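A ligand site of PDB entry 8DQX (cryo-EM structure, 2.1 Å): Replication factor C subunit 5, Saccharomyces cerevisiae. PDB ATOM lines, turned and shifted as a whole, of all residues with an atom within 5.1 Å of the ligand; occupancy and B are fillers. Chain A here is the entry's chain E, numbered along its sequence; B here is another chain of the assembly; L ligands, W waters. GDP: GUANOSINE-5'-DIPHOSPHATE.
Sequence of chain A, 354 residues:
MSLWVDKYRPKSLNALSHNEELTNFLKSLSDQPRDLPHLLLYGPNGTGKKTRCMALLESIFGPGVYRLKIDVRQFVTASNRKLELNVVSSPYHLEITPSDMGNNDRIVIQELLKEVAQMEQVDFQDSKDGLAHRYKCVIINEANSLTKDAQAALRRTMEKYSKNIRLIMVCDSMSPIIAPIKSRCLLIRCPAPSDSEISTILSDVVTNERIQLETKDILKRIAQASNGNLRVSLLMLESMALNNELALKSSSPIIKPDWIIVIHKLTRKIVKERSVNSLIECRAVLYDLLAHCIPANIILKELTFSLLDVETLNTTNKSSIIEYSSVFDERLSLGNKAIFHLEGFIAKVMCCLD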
ATOM      1  N   VAL A   5       6.551   8.508 -13.890  1.00  0.00           N
ATOM      2  CA  VAL A   5       6.302   9.417 -12.782  1.00  0.00           C
ATOM      3  C   VAL A   5       6.755  10.841 -13.139  1.00  0.00           C
ATOM      4  O   VAL A   5       6.226  11.817 -12.594  1.00  0.00           O
ATOM      5  CB  VAL A   5       7.007   8.909 -11.511  1.00  0.00           C
ATOM      6  CG1 VAL A   5       8.519   9.066 -11.635  1.00  0.00           C
ATOM      7  CG2 VAL A   5       6.478   9.660 -10.285  1.00  0.00           C
ATOM      8  N   ASP A   6       7.727  10.979 -14.026  1.00  0.00           N
ATOM      9  CA  ASP A   6       8.227  12.276 -14.464  1.00  0.00           C
ATOM     10  C   ASP A   6       7.607  12.736 -15.779  1.00  0.00           C
ATOM     11  O   ASP A   6       7.334  13.925 -15.948  1.00  0.00           O
ATOM     12  CB  ASP A   6       9.747  12.236 -14.617  1.00  0.00           C
ATOM     13  CG  ASP A   6      10.454  11.786 -13.347  1.00  0.00           C
ATOM     14  OD1 ASP A   6      10.119  12.296 -12.267  1.00  0.00           O
ATOM     15  OD2 ASP A   6      11.342  10.921 -13.447  1.00  0.00           O
ATOM     16  N   TYR A   8       4.706  12.566 -17.038  1.00  0.00           N
ATOM     17  CA  TYR A   8       3.342  13.093 -16.989  1.00  0.00           C
ATOM     18  C   TYR A   8       3.092  14.003 -15.786  1.00  0.00           C
ATOM     19  O   TYR A   8       1.937  14.257 -15.456  1.00  0.00           O
ATOM     20  CB  TYR A   8       2.338  11.941 -17.008  1.00  0.00           C
ATOM     21  CG  TYR A   8       2.452  11.074 -18.241  1.00  0.00           C
ATOM     22  CD1 TYR A   8       1.919  11.483 -19.454  1.00  0.00           C
ATOM     23  CD2 TYR A   8       3.101   9.841 -18.193  1.00  0.00           C
ATOM     24  CE1 TYR A   8       2.022  10.702 -20.588  1.00  0.00           C
ATOM     25  CE2 TYR A   8       3.204   9.052 -19.322  1.00  0.00           C
ATOM     26  CZ  TYR A   8       2.669   9.485 -20.515  1.00  0.00           C
ATOM     27  OH  TYR A   8       2.771   8.701 -21.636  1.00  0.00           O
ATOM     28  N   ARG A   9       4.151  14.491 -15.134  1.00  0.00           N
ATOM     29  CA  ARG A   9       3.960  15.395 -14.005  1.00  0.00           C
ATOM     30  C   ARG A   9       3.327  16.712 -14.485  1.00  0.00           C
ATOM     31  O   ARG A   9       3.817  17.290 -15.467  1.00  0.00           O
ATOM     32  CB  ARG A   9       5.290  15.677 -13.300  1.00  0.00           C
ATOM     33  CG  ARG A   9       5.176  16.637 -12.126  1.00  0.00           C
ATOM     34  CD  ARG A   9       6.400  16.601 -11.206  1.00  0.00           C
ATOM     35  NE  ARG A   9       7.661  16.610 -11.930  1.00  0.00           N
ATOM     36  CZ  ARG A   9       8.480  15.572 -12.071  1.00  0.00           C
ATOM     37  NH1 ARG A   9       8.193  14.393 -11.542  1.00  0.00           N
ATOM     38  NH2 ARG A   9       9.598  15.716 -12.755  1.00  0.00           N
ATOM     39  N   PRO A  10       2.261  17.195 -13.851  1.00  0.00           N
ATOM     40  CA  PRO A  10       1.625  18.431 -14.328  1.00  0.00           C
ATOM     41  C   PRO A  10       2.499  19.662 -14.147  1.00  0.00           C
ATOM     42  O   PRO A  10       3.302  19.760 -13.216  1.00  0.00           O
ATOM     43  CB  PRO A  10       0.341  18.539 -13.478  1.00  0.00           C
ATOM     44  CG  PRO A  10       0.473  17.548 -12.391  1.00  0.00           C
ATOM     45  CD  PRO A  10       1.468  16.522 -12.806  1.00  0.00           C
ATOM     46  N   ALA A  15      -3.566  21.878 -14.633  1.00  0.00           N
ATOM     47  CA  ALA A  15      -3.312  20.479 -14.916  1.00  0.00           C
ATOM     48  C   ALA A  15      -3.260  19.607 -13.651  1.00  0.00           C
ATOM     49  O   ALA A  15      -3.074  18.402 -13.767  1.00  0.00           O
ATOM     50  CB  ALA A  15      -1.997  20.327 -15.698  1.00  0.00           C
ATOM     51  N   LEU A  16      -3.415  20.196 -12.471  1.00  0.00           N
ATOM     52  CA  LEU A  16      -3.516  19.393 -11.256  1.00  0.00           C
ATOM     53  C   LEU A  16      -4.814  18.594 -11.270  1.00  0.00           C
ATOM     54  O   LEU A  16      -5.833  19.026 -11.825  1.00  0.00           O
ATOM     55  CB  LEU A  16      -3.458  20.289 -10.023  1.00  0.00           C
ATOM     56  CG  LEU A  16      -2.200  21.138  -9.841  1.00  0.00           C
ATOM     57  CD1 LEU A  16      -2.335  22.016  -8.594  1.00  0.00           C
ATOM     58  CD2 LEU A  16      -0.942  20.274  -9.747  1.00  0.00           C
ATOM     59  N   SER A  17      -4.791  17.409 -10.643  1.00  0.00           N
ATOM     60  CA  SER A  17      -5.902  16.485 -10.808  1.00  0.00           C
ATOM     61  C   SER A  17      -6.314  15.777  -9.509  1.00  0.00           C
ATOM     62  O   SER A  17      -7.027  14.772  -9.566  1.00  0.00           O
ATOM     63  CB  SER A  17      -5.562  15.442 -11.868  1.00  0.00           C
ATOM     64  OG  SER A  17      -4.660  14.458 -11.380  1.00  0.00           O
ATOM     65  N   HIS A  18      -5.895  16.263  -8.343  1.00  0.00           N
ATOM     66  CA  HIS A  18      -6.458  15.782  -7.085  1.00  0.00           C
ATOM     67  C   HIS A  18      -6.485  16.933  -6.084  1.00  0.00           C
ATOM     68  O   HIS A  18      -5.739  17.900  -6.213  1.00  0.00           O
ATOM     69  CB  HIS A  18      -5.688  14.569  -6.549  1.00  0.00           C
ATOM     70  CG  HIS A  18      -4.271  14.859  -6.137  1.00  0.00           C
ATOM     71  ND1 HIS A  18      -3.943  15.325  -4.885  1.00  0.00           N
ATOM     72  CD2 HIS A  18      -3.102  14.702  -6.801  1.00  0.00           C
ATOM     73  CE1 HIS A  18      -2.640  15.470  -4.798  1.00  0.00           C
ATOM     74  NE2 HIS A  18      -2.101  15.100  -5.944  1.00  0.00           N
ATOM     75  N   PRO A  44       1.907  14.579   3.775  1.00  0.00           N
ATOM     76  CA  PRO A  44       2.636  13.304   3.656  1.00  0.00           C
ATOM     77  C   PRO A  44       3.489  13.257   2.398  1.00  0.00           C
ATOM     78  O   PRO A  44       3.256  13.962   1.423  1.00  0.00           O
ATOM     79  CB  PRO A  44       1.527  12.243   3.614  1.00  0.00           C
ATOM     80  CG  PRO A  44       0.239  12.948   3.809  1.00  0.00           C
ATOM     81  CD  PRO A  44       0.452  14.409   3.604  1.00  0.00           C
ATOM     82  N   ASN A  45       4.491  12.375   2.440  1.00  0.00           N
ATOM     83  CA  ASN A  45       5.452  12.269   1.351  1.00  0.00           C
ATOM     84  C   ASN A  45       4.769  11.842   0.047  1.00  0.00           C
ATOM     85  O   ASN A  45       3.822  11.063   0.046  1.00  0.00           O
ATOM     86  CB  ASN A  45       6.555  11.263   1.685  1.00  0.00           C
ATOM     87  CG  ASN A  45       7.391  11.683   2.891  1.00  0.00           C
ATOM     88  OD1 ASN A  45       6.898  11.712   4.009  1.00  0.00           O
ATOM     89  ND2 ASN A  45       8.659  12.031   2.654  1.00  0.00           N
ATOM     90  N   GLY A  46       5.274  12.384  -1.065  1.00  0.00           N
ATOM     91  CA  GLY A  46       4.894  11.896  -2.380  1.00  0.00           C
ATOM     92  C   GLY A  46       3.472  12.204  -2.804  1.00  0.00           C
ATOM     93  O   GLY A  46       2.914  11.482  -3.633  1.00  0.00           O
ATOM     94  N   THR A  47       2.864  13.251  -2.253  1.00  0.00           N
ATOM     95  CA  THR A  47       1.484  13.592  -2.598  1.00  0.00           C
ATOM     96  C   THR A  47       1.379  14.708  -3.632  1.00  0.00           C
ATOM     97  O   THR A  47       0.297  14.871  -4.212  1.00  0.00           O
ATOM     98  CB  THR A  47       0.701  14.009  -1.343  1.00  0.00           C
ATOM     99  OG1 THR A  47       1.247  15.216  -0.801  1.00  0.00           O
ATOM    100  CG2 THR A  47       0.764  12.909  -0.289  1.00  0.00           C
ATOM    101  N   GLY A  48       2.447  15.450  -3.880  1.00  0.00           N
ATOM    102  CA  GLY A  48       2.418  16.503  -4.888  1.00  0.00           C
ATOM    103  C   GLY A  48       2.718  17.893  -4.360  1.00  0.00           C
ATOM    104  O   GLY A  48       2.281  18.886  -4.945  1.00  0.00           O
ATOM    105  N   LYS A  49       3.469  17.982  -3.262  1.00  0.00           N
ATOM    106  CA  LYS A  49       3.769  19.284  -2.665  1.00  0.00           C
ATOM    107  C   LYS A  49       4.688  20.106  -3.565  1.00  0.00           C
ATOM    108  O   LYS A  49       4.409  21.277  -3.841  1.00  0.00           O
ATOM    109  CB  LYS A  49       4.377  19.105  -1.281  1.00  0.00           C
ATOM    110  CG  LYS A  49       3.396  18.605  -0.236  1.00  0.00           C
ATOM    111  CD  LYS A  49       3.975  18.623   1.174  1.00  0.00           C
ATOM    112  CE  LYS A  49       5.229  17.753   1.295  1.00  0.00           C
ATOM    113  NZ  LYS A  49       5.018  16.366   0.786  1.00  0.00           N
ATOM    114  N   LYS A  50       5.782  19.507  -4.039  1.00  0.00           N
ATOM    115  CA  LYS A  50       6.696  20.237  -4.916  1.00  0.00           C
ATOM    116  C   LYS A  50       6.057  20.519  -6.274  1.00  0.00           C
ATOM    117  O   LYS A  50       6.278  21.587  -6.859  1.00  0.00           O
ATOM    118  CB  LYS A  50       7.998  19.454  -5.083  1.00  0.00           C
ATOM    119  CG  LYS A  50       8.907  19.526  -3.873  1.00  0.00           C
ATOM    120  CD  LYS A  50      10.309  19.063  -4.210  1.00  0.00           C
ATOM    121  CE  LYS A  50      10.334  17.578  -4.535  1.00  0.00           C
ATOM    122  NZ  LYS A  50      11.642  16.985  -4.227  1.00  0.00           N
ATOM    123  N   THR A  51       5.261  19.572  -6.782  1.00  0.00           N
ATOM    124  CA  THR A  51       4.492  19.828  -7.994  1.00  0.00           C
ATOM    125  C   THR A  51       3.648  21.082  -7.851  1.00  0.00           C
ATOM    126  O   THR A  51       3.599  21.928  -8.741  1.00  0.00           O
ATOM    127  CB  THR A  51       3.617  18.609  -8.326  1.00  0.00           C
ATOM    128  OG1 THR A  51       4.438  17.455  -8.501  1.00  0.00           O
ATOM    129  CG2 THR A  51       2.794  18.847  -9.593  1.00  0.00           C
ATOM    130  N   ARG A  52       3.001  21.238  -6.688  1.00  0.00           N
ATOM    131  CA  ARG A  52       2.126  22.383  -6.478  1.00  0.00           C
ATOM    132  C   ARG A  52       2.924  23.668  -6.244  1.00  0.00           C
ATOM    133  O   ARG A  52       2.499  24.739  -6.665  1.00  0.00           O
ATOM    134  CB  ARG A  52       1.185  22.115  -5.303  1.00  0.00           C
ATOM    135  CG  ARG A  52      -0.137  21.496  -5.733  1.00  0.00           C
ATOM    136  CD  ARG A  52      -0.661  20.485  -4.729  1.00  0.00           C
ATOM    137  NE  ARG A  52      -1.748  19.696  -5.299  1.00  0.00           N
ATOM    138  CZ  ARG A  52      -1.582  18.658  -6.096  1.00  0.00           C
ATOM    139  NH1 ARG A  52      -0.374  18.205  -6.412  1.00  0.00           N
ATOM    140  NH2 ARG A  52      -2.653  18.050  -6.600  1.00  0.00           N
ATOM    141  N   ILE A 201      -5.438   8.778 -12.143  1.00  0.00           N
ATOM    142  CA  ILE A 201      -4.123   9.169 -12.664  1.00  0.00           C
ATOM    143  C   ILE A 201      -3.426   7.969 -13.311  1.00  0.00           C
ATOM    144  O   ILE A 201      -2.910   8.056 -14.430  1.00  0.00           O
ATOM    145  CB  ILE A 201      -3.273   9.779 -11.531  1.00  0.00           C
ATOM    146  CG1 ILE A 201      -3.856  11.141 -11.117  1.00  0.00           C
ATOM    147  CG2 ILE A 201      -1.826   9.915 -11.946  1.00  0.00           C
ATOM    148  CD1 ILE A 201      -3.476  11.582  -9.725  1.00  0.00           C
ATOM    149  N   LEU A 230       1.579   8.936  -4.098  1.00  0.00           N
ATOM    150  CA  LEU A 230       1.326   8.917  -5.531  1.00  0.00           C
ATOM    151  C   LEU A 230       2.607   8.622  -6.321  1.00  0.00           C
ATOM    152  O   LEU A 230       2.565   7.899  -7.330  1.00  0.00           O
ATOM    153  CB  LEU A 230       0.716  10.251  -5.960  1.00  0.00           C
ATOM    154  CG  LEU A 230       0.362  10.471  -7.426  1.00  0.00           C
ATOM    155  CD1 LEU A 230      -0.586   9.397  -7.954  1.00  0.00           C
ATOM    156  CD2 LEU A 230      -0.248  11.856  -7.602  1.00  0.00           C
ATOM    157  N   ARG A 231       3.745   9.158  -5.883  1.00  0.00           N
ATOM    158  CA  ARG A 231       5.015   8.825  -6.507  1.00  0.00           C
ATOM    159  C   ARG A 231       5.254   7.315  -6.459  1.00  0.00           C
ATOM    160  O   ARG A 231       5.618   6.695  -7.464  1.00  0.00           O
ATOM    161  CB  ARG A 231       6.144   9.577  -5.802  1.00  0.00           C
ATOM    162  CG  ARG A 231       7.548   9.104  -6.156  1.00  0.00           C
ATOM    163  CD  ARG A 231       8.616  10.097  -5.718  1.00  0.00           C
ATOM    164  NE  ARG A 231       8.718  10.191  -4.266  1.00  0.00           N
ATOM    165  CZ  ARG A 231       8.577  11.308  -3.565  1.00  0.00           C
ATOM    166  NH1 ARG A 231       8.325  12.474  -4.145  1.00  0.00           N
ATOM    167  NH2 ARG A 231       8.702  11.257  -2.244  1.00  0.00           N
ATOM    168  N   LEU A 234       2.913   5.456  -8.962  1.00  0.00           N
ATOM    169  CA  LEU A 234       3.313   5.542 -10.366  1.00  0.00           C
ATOM    170  C   LEU A 234       4.557   4.696 -10.642  1.00  0.00           C
ATOM    171  O   LEU A 234       4.627   3.982 -11.656  1.00  0.00           O
ATOM    172  CB  LEU A 234       3.548   7.006 -10.750  1.00  0.00           C
ATOM    173  CG  LEU A 234       2.268   7.842 -10.912  1.00  0.00           C
ATOM    174  CD1 LEU A 234       2.545   9.309 -10.661  1.00  0.00           C
ATOM    175  CD2 LEU A 234       1.650   7.635 -12.289  1.00  0.00           C
ATOM    176  N   SER B 695      11.414  14.495  -9.394  1.00  0.00           N
ATOM    177  CA  SER B 695      10.784  15.345  -8.385  1.00  0.00           C
ATOM    178  C   SER B 695      10.840  14.583  -7.059  1.00  0.00           C
ATOM    179  O   SER B 695       9.947  13.795  -6.762  1.00  0.00           O
ATOM    180  CB  SER B 695       9.351  15.727  -8.787  1.00  0.00           C
ATOM    181  OG  SER B 695       8.669  16.355  -7.726  1.00  0.00           O
ATOM    182  N   THR B 696      11.888  14.818  -6.284  1.00  0.00           N
ATOM    183  CA  THR B 696      12.116  14.096  -5.036  1.00  0.00           C
ATOM    184  C   THR B 696      13.355  14.643  -4.355  1.00  0.00           C
ATOM    185  O   THR B 696      14.195  15.302  -4.980  1.00  0.00           O
ATOM    186  CB  THR B 696      12.292  12.586  -5.280  1.00  0.00           C
ATOM    187  OG1 THR B 696      12.420  11.899  -4.030  1.00  0.00           O
ATOM    188  CG2 THR B 696      13.532  12.313  -6.137  1.00  0.00           C
ATOM    189  N   TYR B 705      12.767   5.697  -6.386  1.00  0.00           N
ATOM    190  CA  TYR B 705      13.157   5.734  -7.796  1.00  0.00           C
ATOM    191  C   TYR B 705      14.103   4.588  -8.164  1.00  0.00           C
ATOM    192  O   TYR B 705      13.899   3.899  -9.165  1.00  0.00           O
ATOM    193  CB  TYR B 705      13.814   7.077  -8.115  1.00  0.00           C
ATOM    194  CG  TYR B 705      12.871   8.177  -8.575  1.00  0.00           C
ATOM    195  CD1 TYR B 705      12.284   9.043  -7.667  1.00  0.00           C
ATOM    196  CD2 TYR B 705      12.613   8.373  -9.931  1.00  0.00           C
ATOM    197  CE1 TYR B 705      11.444  10.062  -8.088  1.00  0.00           C
ATOM    198  CE2 TYR B 705      11.784   9.386 -10.359  1.00  0.00           C
ATOM    199  CZ  TYR B 705      11.204  10.227  -9.435  1.00  0.00           C
ATOM    200  OH  TYR B 705      10.374  11.246  -9.854  1.00  0.00           O
HETATM  201  PB  GDP L   1       6.015  15.617  -2.723  1.00  0.00           P
HETATM  202  O1B GDP L   1       4.792  15.930  -1.914  1.00  0.00           O
HETATM  203  O2B GDP L   1       6.936  14.709  -1.960  1.00  0.00           O
HETATM  204  O3B GDP L   1       6.735  16.901  -3.070  1.00  0.00           O
HETATM  205  O3A GDP L   1       5.533  14.835  -4.089  1.00  0.00           O
HETATM  206  PA  GDP L   1       5.719  15.356  -5.627  1.00  0.00           P
HETATM  207  O1A GDP L   1       5.337  16.805  -5.760  1.00  0.00           O
HETATM  208  O2A GDP L   1       7.157  15.178  -6.034  1.00  0.00           O
HETATM  209  O5' GDP L   1       4.737  14.436  -6.578  1.00  0.00           O
HETATM  210  C5' GDP L   1       5.098  13.124  -6.893  1.00  0.00           C
HETATM  211  C4' GDP L   1       4.641  12.773  -8.303  1.00  0.00           C
HETATM  212  O4' GDP L   1       3.036  12.610  -8.317  1.00  0.00           O
HETATM  213  C3' GDP L   1       4.925  13.716  -9.171  1.00  0.00           C
HETATM  214  O3' GDP L   1       6.231  13.428  -9.832  1.00  0.00           O
HETATM  215  C2' GDP L   1       3.783  13.661 -10.203  1.00  0.00           C
HETATM  216  O2' GDP L   1       4.109  12.800 -11.202  1.00  0.00           O
HETATM  217  C1' GDP L   1       2.573  13.126  -9.423  1.00  0.00           C
HETATM  218  N9  GDP L   1       1.585  14.164  -9.063  1.00  0.00           N
HETATM  219  C8  GDP L   1       1.552  14.989  -7.996  1.00  0.00           C
HETATM  220  N7  GDP L   1       0.424  15.721  -8.111  1.00  0.00           N
HETATM  221  C5  GDP L   1      -0.212  15.357  -9.212  1.00  0.00           C
HETATM  222  C6  GDP L   1      -1.520  15.832  -9.861  1.00  0.00           C
HETATM  223  O6  GDP L   1      -2.159  16.684  -9.343  1.00  0.00           O
HETATM  224  N1  GDP L   1      -1.966  15.243 -11.083  1.00  0.00           N
HETATM  225  C2  GDP L   1      -1.188  14.210 -11.696  1.00  0.00           C
HETATM  226  N2  GDP L   1      -1.642  13.602 -12.931  1.00  0.00           N
HETATM  227  N3  GDP L   1       0.054  13.757 -11.080  1.00  0.00           N
HETATM  228  C4  GDP L   1       0.515  14.372  -9.814  1.00  0.00           C
HETATM  229  O   HOH W   1       0.346  11.852 -14.169  1.00  0.00           O
HETATM  230  O   HOH W   2       3.451  11.492 -13.514  1.00  0.00           O
HETATM  231  O   HOH W   3       7.772  15.283   0.721  1.00  0.00           O
HETATM  232  O   HOH W   4       8.038  12.226  -8.164  1.00  0.00           O
HETATM  233  O   HOH W   5       8.276  17.581  -0.916  1.00  0.00           O
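An oxygen (O1A) of the ligand is in hydrogen-bond range of the side-chain hydroxyl (OG1) of Thr 51, at 3.0 Å. NH1 of Arg 231 is in salt-bridge range of O2B of the ligand (3.4 Å). N of Gly 46 is in hydrogen-bond range of O2B of the ligand (3.0 Å). N of Lys 50 is in hydrogen-bond range of O3B of the ligand. An oxygen (O1B) of the ligand sits at hydrogen-bond distance from the backbone NH of Gly 48, 3.1 Å away. N7 of the ligand is in hydrogen-bond range of NE2 of His 18. The guanidinium group (NH1) of Arg 9 lies within hydrogen-bond range of an oxygen (O3') of the ligand (2.8 Å). The backbone NH (N) of Lys 49 lies within hydrogen-bond range of an oxygen (O1B) of the ligand, 2.8 Å away. The backbone NH (N) of Thr 47 sits at hydrogen-bond distance from an oxygen (O1B) of the ligand. The backbone carbonyl oxygen (O) of Val 5 lies within hydrogen-bond range of an oxygen (O2') of the ligand (2.7 Å). N of Ser 17 is in hydrogen-bond range of O6 of the ligand, 3.0 Å away. NZ of Lys 49 lies within salt-bridge range of O1B of the ligand, 2.7 Å away. The backbone NH of Thr 51 sits at hydrogen-bond distance from an oxygen (O1A) of the ligand. The guanidinium group (NH2) of Arg 52 sits at hydrogen-bond distance from an oxygen (O6) of the ligand. OG of Ser 17 sits at hydrogen-bond distance from N1 of the ligand (2.8 Å). The side-chain hydroxyl (OG) of Ser 695 of chain B lies within hydrogen-bond range of an oxygen (O2A) of the ligand (2.6 Å).
The backbone NH of Leu 230 sits at hydrogen-bond distance from the backbone carbonyl oxygen of Gly 46 (2.9 Å). The side-chain hydroxyl of Tyr 705 of chain B sits at hydrogen-bond distance from the backbone NH of Ser 695 of chain B, at 3.4 Å. NH1 of Arg 9 is in salt-bridge range of OD1 of Asp 6 (2.9 Å). NH2 of Arg 52 lies within hydrogen-bond range of NE2 of His 18. O of Ser 695 of chain B lies within hydrogen-bond range of NH1 of Arg 231, 3.4 Å away. O of Val 5 is in hydrogen-bond range of NH1 of Arg 9, 3.4 Å away. NZ of Lys 50 sits close to O of Thr 696 of chain B, at 3.1 Å. O of Thr 47 lies within hydrogen-bond range of NE2 of His 18 (3.0 Å).
Water W2 lies within hydrogen-bond range of O2' of the ligand, O of Val 5 and N of Arg 9. Water W4 lies within hydrogen-bond range of O3' of the ligand (2.7 Å), O of Ser 695 of chain B (2.8 Å) and OH of Tyr 705 of chain B (3.0 Å). Water W3 lies within hydrogen-bond range of O2B of the ligand and NZ of Lys 49. Water W1 lies within hydrogen-bond range of a nitrogen (N2) of the ligand (2.9 Å) and the backbone carbonyl oxygen of Tyr 8 (3.2 Å).
Pro 10 touches the ligand. CA of Leu 16 touches O6 of the ligand, 3.6 Å away. CG1 of Ile 201 touches N2 of the ligand, 3.8 Å away. Leu 230 touches the ligand (CD2 to N9, 3.3 Å). Leu 234 touches the ligand. Hydrophobic or aromatic side chains within 4 Å of the ligand: Val 5, Pro 10, Leu 16, His 18, Ile 201, Leu 230 and Leu 234. Within 4 Å of the ligand: Val 5, Arg 9, Pro 10, Leu 16, Ser 17, His 18, Gly 46, Thr 47, Gly 48, Lys 49, Lys 50, Thr 51, Arg 52, Ile 201, Leu 230, Arg 231, Leu 234 and Ser 695 of chain B. The nearest printed residue that does not touch the ligand is Asn 45 (4.1 Å).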
